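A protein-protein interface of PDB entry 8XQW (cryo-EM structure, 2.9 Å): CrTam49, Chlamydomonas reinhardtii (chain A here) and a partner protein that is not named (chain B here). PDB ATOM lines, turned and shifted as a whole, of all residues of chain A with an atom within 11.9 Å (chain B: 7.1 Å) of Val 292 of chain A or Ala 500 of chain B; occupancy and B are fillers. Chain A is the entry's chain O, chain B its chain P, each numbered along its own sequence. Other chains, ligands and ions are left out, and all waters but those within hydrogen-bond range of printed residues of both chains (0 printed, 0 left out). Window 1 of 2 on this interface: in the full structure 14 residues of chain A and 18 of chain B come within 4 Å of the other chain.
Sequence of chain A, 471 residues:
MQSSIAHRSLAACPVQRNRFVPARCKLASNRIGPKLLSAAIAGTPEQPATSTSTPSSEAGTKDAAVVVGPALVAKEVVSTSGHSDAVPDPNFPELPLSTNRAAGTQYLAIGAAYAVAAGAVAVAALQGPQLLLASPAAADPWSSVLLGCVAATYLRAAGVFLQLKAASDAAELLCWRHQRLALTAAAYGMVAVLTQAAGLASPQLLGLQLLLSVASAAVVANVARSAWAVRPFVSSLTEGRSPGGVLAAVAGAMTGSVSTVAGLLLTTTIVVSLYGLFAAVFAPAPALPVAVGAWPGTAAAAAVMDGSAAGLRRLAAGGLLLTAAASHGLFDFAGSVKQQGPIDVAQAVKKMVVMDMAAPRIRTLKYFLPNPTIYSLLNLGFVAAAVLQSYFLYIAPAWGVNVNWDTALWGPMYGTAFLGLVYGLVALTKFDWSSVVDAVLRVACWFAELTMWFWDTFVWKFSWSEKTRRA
Val 292 of chain A touches just these residues of chain B: Ala 500 (3.7 Å) and Ser 504 (3.9 Å). Of the printed residues of chain B, Gly 293 of chain A touches Val 283 (3.5 Å), Ala 500 (3.5 Å) and Arg 503 (2.8 Å). Of the printed residues of chain B, Trp 295 of chain A touches Met 489 and Arg 503. Of the printed residues of chain B, Pro 296 of chain A touches Val 283 (3.0 Å). Of the printed residues of chain A, Val 283 of chain B touches Gly 293 and Pro 296. Of chain A, only Trp 295 comes within 4 Å of Met 489 of chain B. Leu 498 of chain B touches none of the printed residues of chain A. No residue of chain A comes within 4 Å of Ala 499 of chain B. Ala 500 of chain B touches just these residues of chain A: Val 292 (3.7 Å) and Gly 293 (3.5 Å). No residue of chain A comes within 4 Å of Ala 502 of chain B. Of the printed residues of chain A, Arg 503 of chain B touches Gly 293 (2.8 Å) and Trp 295 (3.1 Å). Ser 504 of chain B touches just one residue of chain A: Val 292 (3.9 Å). The nearest residue of chain B that does not touch Val 292 of chain A is Val 283 of chain B (4.9 Å). The nearest residue of chain A that does not touch Ala 500 of chain B is Ala 294 of chain A (4.1 Å). The nearest printed residue of chain A that does not touch Val 283 of chain B is Val 292 of chain A (4.9 Å).
The guanidinium group (NH1) of Arg 503 of chain B sits close to the backbone NH (N) of Trp 295 of chain A (3.1 Å). O of Gly 293 of chain A is in hydrogen-bond range of NH1 of Arg 503 of chain B (2.8 Å).
Ala 500 of chain B touches Val 292 of chain A. Val 292 of chain A touches Ser 504 of chain B. CA of Gly 293 of chain A touches CG1 of Val 283 of chain B (3.5 Å). Gly 293 of chain A touches Ala 500 of chain B (O to CA, 3.5 Å). Trp 295 of chain A touches Met 489 of chain B (CZ3 to O, 3.8 Å). Pro 296 of chain A touches Val 283 of chain B (CB to O, 3.0 Å).
Printed residues of chain A that touch a printed residue of chain B: Val 292, Gly 293, Trp 295 and Pro 296. Of the 19 printed residues of chain B, 5 touch a printed residue of chain A. Among the printed residues, no Asp or Glu carboxylate lies within 4 Å of a Lys or Arg side-chain nitrogen of the other chain.
O of Met 489 of chain B lies within hydrogen-bond range of NH2 of Arg 503 of chain B, 3.0 Å away. The backbone carbonyl oxygen of Ala 500 of chain B lies within hydrogen-bond range of the side-chain hydroxyl of Ser 504 of chain B, at 2.6 Å.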
ATOM      1  N   ALA A 287     -24.208  34.512  13.891  1.00  0.00           N
ATOM      2  CA  ALA A 287     -23.766  33.145  14.116  1.00  0.00           C
ATOM      3  C   ALA A 287     -22.590  33.156  15.082  1.00  0.00           C
ATOM      4  O   ALA A 287     -21.606  33.873  14.880  1.00  0.00           O
ATOM      5  CB  ALA A 287     -23.378  32.455  12.802  1.00  0.00           C
ATOM      6  N   LEU A 288     -22.703  32.349  16.135  1.00  0.00           N
ATOM      7  CA  LEU A 288     -21.716  32.328  17.201  1.00  0.00           C
ATOM      8  C   LEU A 288     -20.376  31.787  16.701  1.00  0.00           C
ATOM      9  O   LEU A 288     -20.314  31.107  15.675  1.00  0.00           O
ATOM     10  CB  LEU A 288     -22.206  31.471  18.361  1.00  0.00           C
ATOM     11  CG  LEU A 288     -22.820  32.232  19.533  1.00  0.00           C
ATOM     12  CD1 LEU A 288     -24.205  32.729  19.166  1.00  0.00           C
ATOM     13  CD2 LEU A 288     -22.870  31.355  20.766  1.00  0.00           C
ATOM     14  N   PRO A 289     -19.286  32.091  17.407  1.00  0.00           N
ATOM     15  CA  PRO A 289     -17.990  31.506  17.045  1.00  0.00           C
ATOM     16  C   PRO A 289     -18.022  29.988  17.144  1.00  0.00           C
ATOM     17  O   PRO A 289     -18.610  29.418  18.066  1.00  0.00           O
ATOM     18  CB  PRO A 289     -17.026  32.115  18.067  1.00  0.00           C
ATOM     19  CG  PRO A 289     -17.693  33.367  18.518  1.00  0.00           C
ATOM     20  CD  PRO A 289     -19.161  33.093  18.480  1.00  0.00           C
ATOM     21  N   VAL A 290     -17.372  29.334  16.180  1.00  0.00           N
ATOM     22  CA  VAL A 290     -17.414  27.877  16.121  1.00  0.00           C
ATOM     23  C   VAL A 290     -16.508  27.262  17.182  1.00  0.00           C
ATOM     24  O   VAL A 290     -16.927  26.362  17.919  1.00  0.00           O
ATOM     25  CB  VAL A 290     -17.061  27.389  14.702  1.00  0.00           C
ATOM     26  CG1 VAL A 290     -15.770  28.025  14.201  1.00  0.00           C
ATOM     27  CG2 VAL A 290     -16.973  25.869  14.666  1.00  0.00           C
ATOM     28  N   ALA A 291     -15.269  27.743  17.297  1.00  0.00           N
ATOM     29  CA  ALA A 291     -14.277  27.189  18.221  1.00  0.00           C
ATOM     30  C   ALA A 291     -14.085  25.691  17.966  1.00  0.00           C
ATOM     31  O   ALA A 291     -14.416  24.837  18.788  1.00  0.00           O
ATOM     32  CB  ALA A 291     -14.666  27.458  19.680  1.00  0.00           C
ATOM     33  N   VAL A 292     -13.547  25.412  16.775  1.00  0.00           N
ATOM     34  CA  VAL A 292     -13.392  24.045  16.287  1.00  0.00           C
ATOM     35  C   VAL A 292     -12.722  23.177  17.339  1.00  0.00           C
ATOM     36  O   VAL A 292     -11.677  23.536  17.892  1.00  0.00           O
ATOM     37  CB  VAL A 292     -12.593  24.048  14.972  1.00  0.00           C
ATOM     38  CG1 VAL A 292     -12.093  22.652  14.646  1.00  0.00           C
ATOM     39  CG2 VAL A 292     -13.442  24.594  13.844  1.00  0.00           C
ATOM     40  N   GLY A 293     -13.329  22.027  17.620  1.00  0.00           N
ATOM     41  CA  GLY A 293     -12.779  21.080  18.567  1.00  0.00           C
ATOM     42  C   GLY A 293     -13.278  21.217  19.982  1.00  0.00           C
ATOM     43  O   GLY A 293     -12.647  20.680  20.900  1.00  0.00           O
ATOM     44  N   ALA A 294     -14.393  21.907  20.196  1.00  0.00           N
ATOM     45  CA  ALA A 294     -14.890  22.205  21.535  1.00  0.00           C
ATOM     46  C   ALA A 294     -15.856  21.107  21.959  1.00  0.00           C
ATOM     47  O   ALA A 294     -17.051  21.176  21.669  1.00  0.00           O
ATOM     48  CB  ALA A 294     -15.558  23.574  21.571  1.00  0.00           C
ATOM     49  N   TRP A 295     -15.326  20.091  22.647  1.00  0.00           N
ATOM     50  CA  TRP A 295     -16.096  19.003  23.245  1.00  0.00           C
ATOM     51  C   TRP A 295     -17.164  18.461  22.305  1.00  0.00           C
ATOM     52  O   TRP A 295     -18.346  18.789  22.464  1.00  0.00           O
ATOM     53  CB  TRP A 295     -16.746  19.420  24.561  1.00  0.00           C
ATOM     54  CG  TRP A 295     -17.101  18.209  25.345  1.00  0.00           C
ATOM     55  CD1 TRP A 295     -18.281  17.537  25.315  1.00  0.00           C
ATOM     56  CD2 TRP A 295     -16.246  17.482  26.231  1.00  0.00           C
ATOM     57  NE1 TRP A 295     -18.226  16.448  26.149  1.00  0.00           N
ATOM     58  CE2 TRP A 295     -16.985  16.393  26.723  1.00  0.00           C
ATOM     59  CE3 TRP A 295     -14.930  17.654  26.667  1.00  0.00           C
ATOM     60  CZ2 TRP A 295     -16.455  15.480  27.629  1.00  0.00           C
ATOM     61  CZ3 TRP A 295     -14.406  16.746  27.567  1.00  0.00           C
ATOM     62  CH2 TRP A 295     -15.167  15.673  28.037  1.00  0.00           C
ATOM     63  N   PRO A 296     -16.794  17.636  21.330  1.00  0.00           N
ATOM     64  CA  PRO A 296     -17.728  17.244  20.261  1.00  0.00           C
ATOM     65  C   PRO A 296     -19.082  16.722  20.722  1.00  0.00           C
ATOM     66  O   PRO A 296     -19.954  16.455  19.889  1.00  0.00           O
ATOM     67  CB  PRO A 296     -16.962  16.144  19.517  1.00  0.00           C
ATOM     68  CG  PRO A 296     -15.861  15.729  20.447  1.00  0.00           C
ATOM     69  CD  PRO A 296     -15.500  16.951  21.206  1.00  0.00           C
ATOM     70  N   GLY A 297     -19.275  16.559  22.026  1.00  0.00           N
ATOM     71  CA  GLY A 297     -20.585  16.205  22.525  1.00  0.00           C
ATOM     72  C   GLY A 297     -21.526  17.387  22.629  1.00  0.00           C
ATOM     73  O   GLY A 297     -21.537  18.272  21.765  1.00  0.00           O
ATOM     74  N   THR A 298     -22.312  17.415  23.695  1.00  0.00           N
ATOM     75  CA  THR A 298     -23.330  18.430  23.919  1.00  0.00           C
ATOM     76  C   THR A 298     -22.717  19.581  24.720  1.00  0.00           C
ATOM     77  O   THR A 298     -21.493  19.718  24.780  1.00  0.00           O
ATOM     78  CB  THR A 298     -24.549  17.800  24.596  1.00  0.00           C
ATOM     79  OG1 THR A 298     -24.653  16.431  24.196  1.00  0.00           O
ATOM     80  CG2 THR A 298     -25.822  18.520  24.163  1.00  0.00           C
ATOM     81  N   ALA A 300     -23.638  22.649  23.778  1.00  0.00           N
ATOM     82  CA  ALA A 300     -23.773  23.680  22.752  1.00  0.00           C
ATOM     83  C   ALA A 300     -22.443  24.198  22.235  1.00  0.00           C
ATOM     84  O   ALA A 300     -22.423  25.174  21.475  1.00  0.00           O
ATOM     85  CB  ALA A 300     -24.612  24.863  23.248  1.00  0.00           C
ATOM     86  N   ALA A 301     -21.331  23.584  22.621  1.00  0.00           N
ATOM     87  CA  ALA A 301     -20.033  24.003  22.122  1.00  0.00           C
ATOM     88  C   ALA A 301     -19.911  23.647  20.647  1.00  0.00           C
ATOM     89  O   ALA A 301     -20.208  22.519  20.239  1.00  0.00           O
ATOM     90  CB  ALA A 301     -18.916  23.346  22.929  1.00  0.00           C
ATOM     91  N   ALA A 302     -19.479  24.624  19.848  1.00  0.00           N
ATOM     92  CA  ALA A 302     -19.434  24.513  18.390  1.00  0.00           C
ATOM     93  C   ALA A 302     -20.822  24.211  17.822  1.00  0.00           C
ATOM     94  O   ALA A 302     -21.062  23.169  17.204  1.00  0.00           O
ATOM     95  CB  ALA A 302     -18.408  23.466  17.941  1.00  0.00           C
ATOM     96  N   ALA A 303     -21.741  25.146  18.045  1.00  0.00           N
ATOM     97  CA  ALA A 303     -23.126  25.011  17.615  1.00  0.00           C
ATOM     98  C   ALA A 303     -23.655  26.357  17.116  1.00  0.00           C
ATOM     99  O   ALA A 303     -22.972  27.382  17.182  1.00  0.00           O
ATOM    100  CB  ALA A 303     -23.982  24.454  18.754  1.00  0.00           C
ATOM    101  N   VAL A 304     -24.923  26.381  16.683  1.00  0.00           N
ATOM    102  CA  VAL A 304     -25.555  27.661  16.219  1.00  0.00           C
ATOM    103  C   VAL A 304     -26.317  28.315  17.387  1.00  0.00           C
ATOM    104  O   VAL A 304     -25.949  28.056  18.552  1.00  0.00           O
ATOM    105  CB  VAL A 304     -26.475  27.462  14.996  1.00  0.00           C
ATOM    106  CG1 VAL A 304     -26.201  28.491  13.907  1.00  0.00           C
ATOM    107  CG2 VAL A 304     -26.384  26.049  14.435  1.00  0.00           C
ATOM    108  N   VAL B 231       0.938  22.648  22.834  1.00  0.00           N
ATOM    109  CA  VAL B 231      -0.351  22.370  22.222  1.00  0.00           C
ATOM    110  C   VAL B 231      -1.379  23.473  22.438  1.00  0.00           C
ATOM    111  O   VAL B 231      -2.207  23.700  21.547  1.00  0.00           O
ATOM    112  CB  VAL B 231      -0.913  21.021  22.709  1.00  0.00           C
ATOM    113  CG1 VAL B 231      -0.144  19.883  22.073  1.00  0.00           C
ATOM    114  CG2 VAL B 231      -0.853  20.942  24.214  1.00  0.00           C
ATOM    115  N   ARG B 280     -11.341  16.845  10.852  1.00  0.00           N
ATOM    116  CA  ARG B 280     -12.633  17.339  11.313  1.00  0.00           C
ATOM    117  C   ARG B 280     -13.591  16.190  11.602  1.00  0.00           C
ATOM    118  O   ARG B 280     -14.366  16.242  12.566  1.00  0.00           O
ATOM    119  CB  ARG B 280     -13.223  18.292  10.278  1.00  0.00           C
ATOM    120  CG  ARG B 280     -12.276  19.408   9.884  1.00  0.00           C
ATOM    121  CD  ARG B 280     -12.429  19.777   8.427  1.00  0.00           C
ATOM    122  NE  ARG B 280     -12.137  18.650   7.549  1.00  0.00           N
ATOM    123  CZ  ARG B 280     -12.231  18.690   6.224  1.00  0.00           C
ATOM    124  NH1 ARG B 280     -12.605  19.808   5.614  1.00  0.00           N
ATOM    125  NH2 ARG B 280     -11.952  17.611   5.507  1.00  0.00           N
ATOM    126  N   VAL B 283     -12.653  14.823  14.848  1.00  0.00           N
ATOM    127  CA  VAL B 283     -12.983  15.737  15.930  1.00  0.00           C
ATOM    128  C   VAL B 283     -14.487  15.758  16.176  1.00  0.00           C
ATOM    129  O   VAL B 283     -14.940  16.102  17.274  1.00  0.00           O
ATOM    130  CB  VAL B 283     -12.410  17.131  15.606  1.00  0.00           C
ATOM    131  CG1 VAL B 283     -12.981  18.200  16.516  1.00  0.00           C
ATOM    132  CG2 VAL B 283     -10.897  17.104  15.724  1.00  0.00           C
ATOM    133  N   TYR B 288     -13.108  10.591  20.571  1.00  0.00           N
ATOM    134  CA  TYR B 288     -11.782  11.194  20.612  1.00  0.00           C
ATOM    135  C   TYR B 288     -11.616  12.070  21.848  1.00  0.00           C
ATOM    136  O   TYR B 288     -10.546  12.089  22.467  1.00  0.00           O
ATOM    137  CB  TYR B 288     -11.551  12.000  19.335  1.00  0.00           C
ATOM    138  CG  TYR B 288     -10.337  12.901  19.344  1.00  0.00           C
ATOM    139  CD1 TYR B 288     -10.402  14.188  19.866  1.00  0.00           C
ATOM    140  CD2 TYR B 288      -9.131  12.477  18.805  1.00  0.00           C
ATOM    141  CE1 TYR B 288      -9.298  15.014  19.871  1.00  0.00           C
ATOM    142  CE2 TYR B 288      -8.021  13.302  18.801  1.00  0.00           C
ATOM    143  CZ  TYR B 288      -8.114  14.568  19.336  1.00  0.00           C
ATOM    144  OH  TYR B 288      -7.019  15.395  19.334  1.00  0.00           O
ATOM    145  N   PHE B 488      -8.401  21.285  32.988  1.00  0.00           N
ATOM    146  CA  PHE B 488      -7.789  21.884  31.809  1.00  0.00           C
ATOM    147  C   PHE B 488      -8.395  21.393  30.500  1.00  0.00           C
ATOM    148  O   PHE B 488      -8.508  22.172  29.551  1.00  0.00           O
ATOM    149  CB  PHE B 488      -6.281  21.631  31.807  1.00  0.00           C
ATOM    150  CG  PHE B 488      -5.564  22.293  32.946  1.00  0.00           C
ATOM    151  CD1 PHE B 488      -5.606  23.663  33.100  1.00  0.00           C
ATOM    152  CD2 PHE B 488      -4.855  21.543  33.864  1.00  0.00           C
ATOM    153  CE1 PHE B 488      -4.960  24.267  34.147  1.00  0.00           C
ATOM    154  CE2 PHE B 488      -4.207  22.146  34.908  1.00  0.00           C
ATOM    155  CZ  PHE B 488      -4.257  23.507  35.049  1.00  0.00           C
ATOM    156  N   MET B 489      -8.803  20.127  30.421  1.00  0.00           N
ATOM    157  CA  MET B 489      -9.274  19.552  29.171  1.00  0.00           C
ATOM    158  C   MET B 489     -10.619  18.853  29.279  1.00  0.00           C
ATOM    159  O   MET B 489     -11.009  18.155  28.335  1.00  0.00           O
ATOM    160  CB  MET B 489      -8.245  18.552  28.628  1.00  0.00           C
ATOM    161  CG  MET B 489      -6.811  19.008  28.745  1.00  0.00           C
ATOM    162  SD  MET B 489      -6.186  19.644  27.190  1.00  0.00           S
ATOM    163  CE  MET B 489      -6.193  18.147  26.213  1.00  0.00           C
ATOM    164  N   PRO B 493     -13.878  23.319  31.409  1.00  0.00           N
ATOM    165  CA  PRO B 493     -12.567  23.624  31.952  1.00  0.00           C
ATOM    166  C   PRO B 493     -12.477  25.036  32.475  1.00  0.00           C
ATOM    167  O   PRO B 493     -13.526  25.670  32.696  1.00  0.00           O
ATOM    168  CB  PRO B 493     -11.752  23.440  30.687  1.00  0.00           C
ATOM    169  CG  PRO B 493     -12.614  24.064  29.616  1.00  0.00           C
ATOM    170  CD  PRO B 493     -14.030  23.686  30.011  1.00  0.00           C
ATOM    171  N   ASP B 495     -10.713  27.389  30.750  1.00  0.00           N
ATOM    172  CA  ASP B 495     -10.799  28.226  29.554  1.00  0.00           C
ATOM    173  C   ASP B 495     -11.001  27.292  28.365  1.00  0.00           C
ATOM    174  O   ASP B 495     -10.198  26.373  28.137  1.00  0.00           O
ATOM    175  CB  ASP B 495      -9.563  29.102  29.371  1.00  0.00           C
ATOM    176  CG  ASP B 495      -9.677  30.028  28.171  1.00  0.00           C
ATOM    177  OD1 ASP B 495      -9.741  29.538  27.027  1.00  0.00           O
ATOM    178  OD2 ASP B 495      -9.719  31.258  28.383  1.00  0.00           O
ATOM    179  N   PRO B 496     -12.058  27.502  27.575  1.00  0.00           N
ATOM    180  CA  PRO B 496     -12.445  26.487  26.581  1.00  0.00           C
ATOM    181  C   PRO B 496     -11.511  26.391  25.386  1.00  0.00           C
ATOM    182  O   PRO B 496     -11.150  25.273  24.984  1.00  0.00           O
ATOM    183  CB  PRO B 496     -13.848  26.942  26.147  1.00  0.00           C
ATOM    184  CG  PRO B 496     -14.249  28.030  27.128  1.00  0.00           C
ATOM    185  CD  PRO B 496     -12.984  28.643  27.593  1.00  0.00           C
ATOM    186  N   GLU B 497     -11.122  27.522  24.796  1.00  0.00           N
ATOM    187  CA  GLU B 497     -10.333  27.470  23.570  1.00  0.00           C
ATOM    188  C   GLU B 497      -8.977  26.828  23.818  1.00  0.00           C
ATOM    189  O   GLU B 497      -8.393  26.228  22.908  1.00  0.00           O
ATOM    190  CB  GLU B 497     -10.174  28.867  22.976  1.00  0.00           C
ATOM    191  CG  GLU B 497      -9.693  29.917  23.951  1.00  0.00           C
ATOM    192  CD  GLU B 497     -10.279  31.286  23.668  1.00  0.00           C
ATOM    193  OE1 GLU B 497      -9.505  32.211  23.350  1.00  0.00           O
ATOM    194  OE2 GLU B 497     -11.512  31.435  23.766  1.00  0.00           O
ATOM    195  N   LEU B 498      -8.471  26.918  25.050  1.00  0.00           N
ATOM    196  CA  LEU B 498      -7.262  26.180  25.395  1.00  0.00           C
ATOM    197  C   LEU B 498      -7.422  24.700  25.082  1.00  0.00           C
ATOM    198  O   LEU B 498      -6.637  24.133  24.313  1.00  0.00           O
ATOM    199  CB  LEU B 498      -6.926  26.371  26.872  1.00  0.00           C
ATOM    200  CG  LEU B 498      -5.550  25.847  27.292  1.00  0.00           C
ATOM    201  CD1 LEU B 498      -4.869  26.837  28.204  1.00  0.00           C
ATOM    202  CD2 LEU B 498      -5.641  24.499  27.969  1.00  0.00           C
ATOM    203  N   ALA B 499      -8.447  24.063  25.648  1.00  0.00           N
ATOM    204  CA  ALA B 499      -8.609  22.626  25.479  1.00  0.00           C
ATOM    205  C   ALA B 499      -9.011  22.275  24.053  1.00  0.00           C
ATOM    206  O   ALA B 499      -8.629  21.218  23.537  1.00  0.00           O
ATOM    207  CB  ALA B 499      -9.632  22.098  26.479  1.00  0.00           C
ATOM    208  N   ALA B 500      -9.767  23.154  23.393  1.00  0.00           N
ATOM    209  CA  ALA B 500     -10.112  22.906  21.995  1.00  0.00           C
ATOM    210  C   ALA B 500      -8.862  22.857  21.123  1.00  0.00           C
ATOM    211  O   ALA B 500      -8.653  21.904  20.355  1.00  0.00           O
ATOM    212  CB  ALA B 500     -11.076  23.980  21.499  1.00  0.00           C
ATOM    213  N   ALA B 501      -8.014  23.884  21.231  1.00  0.00           N
ATOM    214  CA  ALA B 501      -6.774  23.915  20.468  1.00  0.00           C
ATOM    215  C   ALA B 501      -5.854  22.773  20.871  1.00  0.00           C
ATOM    216  O   ALA B 501      -5.117  22.233  20.039  1.00  0.00           O
ATOM    217  CB  ALA B 501      -6.079  25.258  20.668  1.00  0.00           C
ATOM    218  N   ALA B 502      -5.882  22.399  22.150  1.00  0.00           N
ATOM    219  CA  ALA B 502      -5.085  21.270  22.603  1.00  0.00           C
ATOM    220  C   ALA B 502      -5.483  19.999  21.875  1.00  0.00           C
ATOM    221  O   ALA B 502      -4.629  19.302  21.324  1.00  0.00           O
ATOM    222  CB  ALA B 502      -5.235  21.097  24.110  1.00  0.00           C
ATOM    223  N   ARG B 503      -6.779  19.693  21.848  1.00  0.00           N
ATOM    224  CA  ARG B 503      -7.227  18.500  21.138  1.00  0.00           C
ATOM    225  C   ARG B 503      -6.864  18.579  19.661  1.00  0.00           C
ATOM    226  O   ARG B 503      -6.420  17.588  19.068  1.00  0.00           O
ATOM    227  CB  ARG B 503      -8.732  18.309  21.326  1.00  0.00           C
ATOM    228  CG  ARG B 503      -9.151  18.124  22.783  1.00  0.00           C
ATOM    229  CD  ARG B 503     -10.606  17.705  22.931  1.00  0.00           C
ATOM    230  NE  ARG B 503     -11.101  18.010  24.271  1.00  0.00           N
ATOM    231  CZ  ARG B 503     -11.942  19.000  24.552  1.00  0.00           C
ATOM    232  NH1 ARG B 503     -12.398  19.780  23.583  1.00  0.00           N
ATOM    233  NH2 ARG B 503     -12.327  19.209  25.802  1.00  0.00           N
ATOM    234  N   SER B 504      -7.003  19.759  19.059  1.00  0.00           N
ATOM    235  CA  SER B 504      -6.707  19.885  17.636  1.00  0.00           C
ATOM    236  C   SER B 504      -5.236  19.605  17.341  1.00  0.00           C
ATOM    237  O   SER B 504      -4.895  18.662  16.610  1.00  0.00           O
ATOM    238  CB  SER B 504      -7.104  21.274  17.153  1.00  0.00           C
ATOM    239  OG  SER B 504      -8.278  21.705  17.817  1.00  0.00           O
ATOM    240  N   VAL B 505      -4.333  20.407  17.901  1.00  0.00           N
ATOM    241  CA  VAL B 505      -2.934  20.188  17.562  1.00  0.00           C
ATOM    242  C   VAL B 505      -2.368  18.984  18.295  1.00  0.00           C
ATOM    243  O   VAL B 505      -1.169  18.725  18.205  1.00  0.00           O
ATOM    244  CB  VAL B 505      -2.080  21.431  17.838  1.00  0.00           C
ATOM    245  CG1 VAL B 505      -2.580  22.605  17.030  1.00  0.00           C
ATOM    246  CG2 VAL B 505      -2.064  21.727  19.297  1.00  0.00           C
ATOM    247  N   LEU B 506      -3.191  18.259  19.058  1.00  0.00           N
ATOM    248  CA  LEU B 506      -2.770  16.952  19.544  1.00  0.00           C
ATOM    249  C   LEU B 506      -3.128  15.876  18.538  1.00  0.00           C
ATOM    250  O   LEU B 506      -2.450  14.847  18.443  1.00  0.00           O
ATOM    251  CB  LEU B 506      -3.417  16.665  20.896  1.00  0.00           C
ATOM    252  CG  LEU B 506      -2.993  15.388  21.616  1.00  0.00           C
ATOM    253  CD1 LEU B 506      -1.509  15.164  21.459  1.00  0.00           C
ATOM    254  CD2 LEU B 506      -3.364  15.455  23.085  1.00  0.00           C
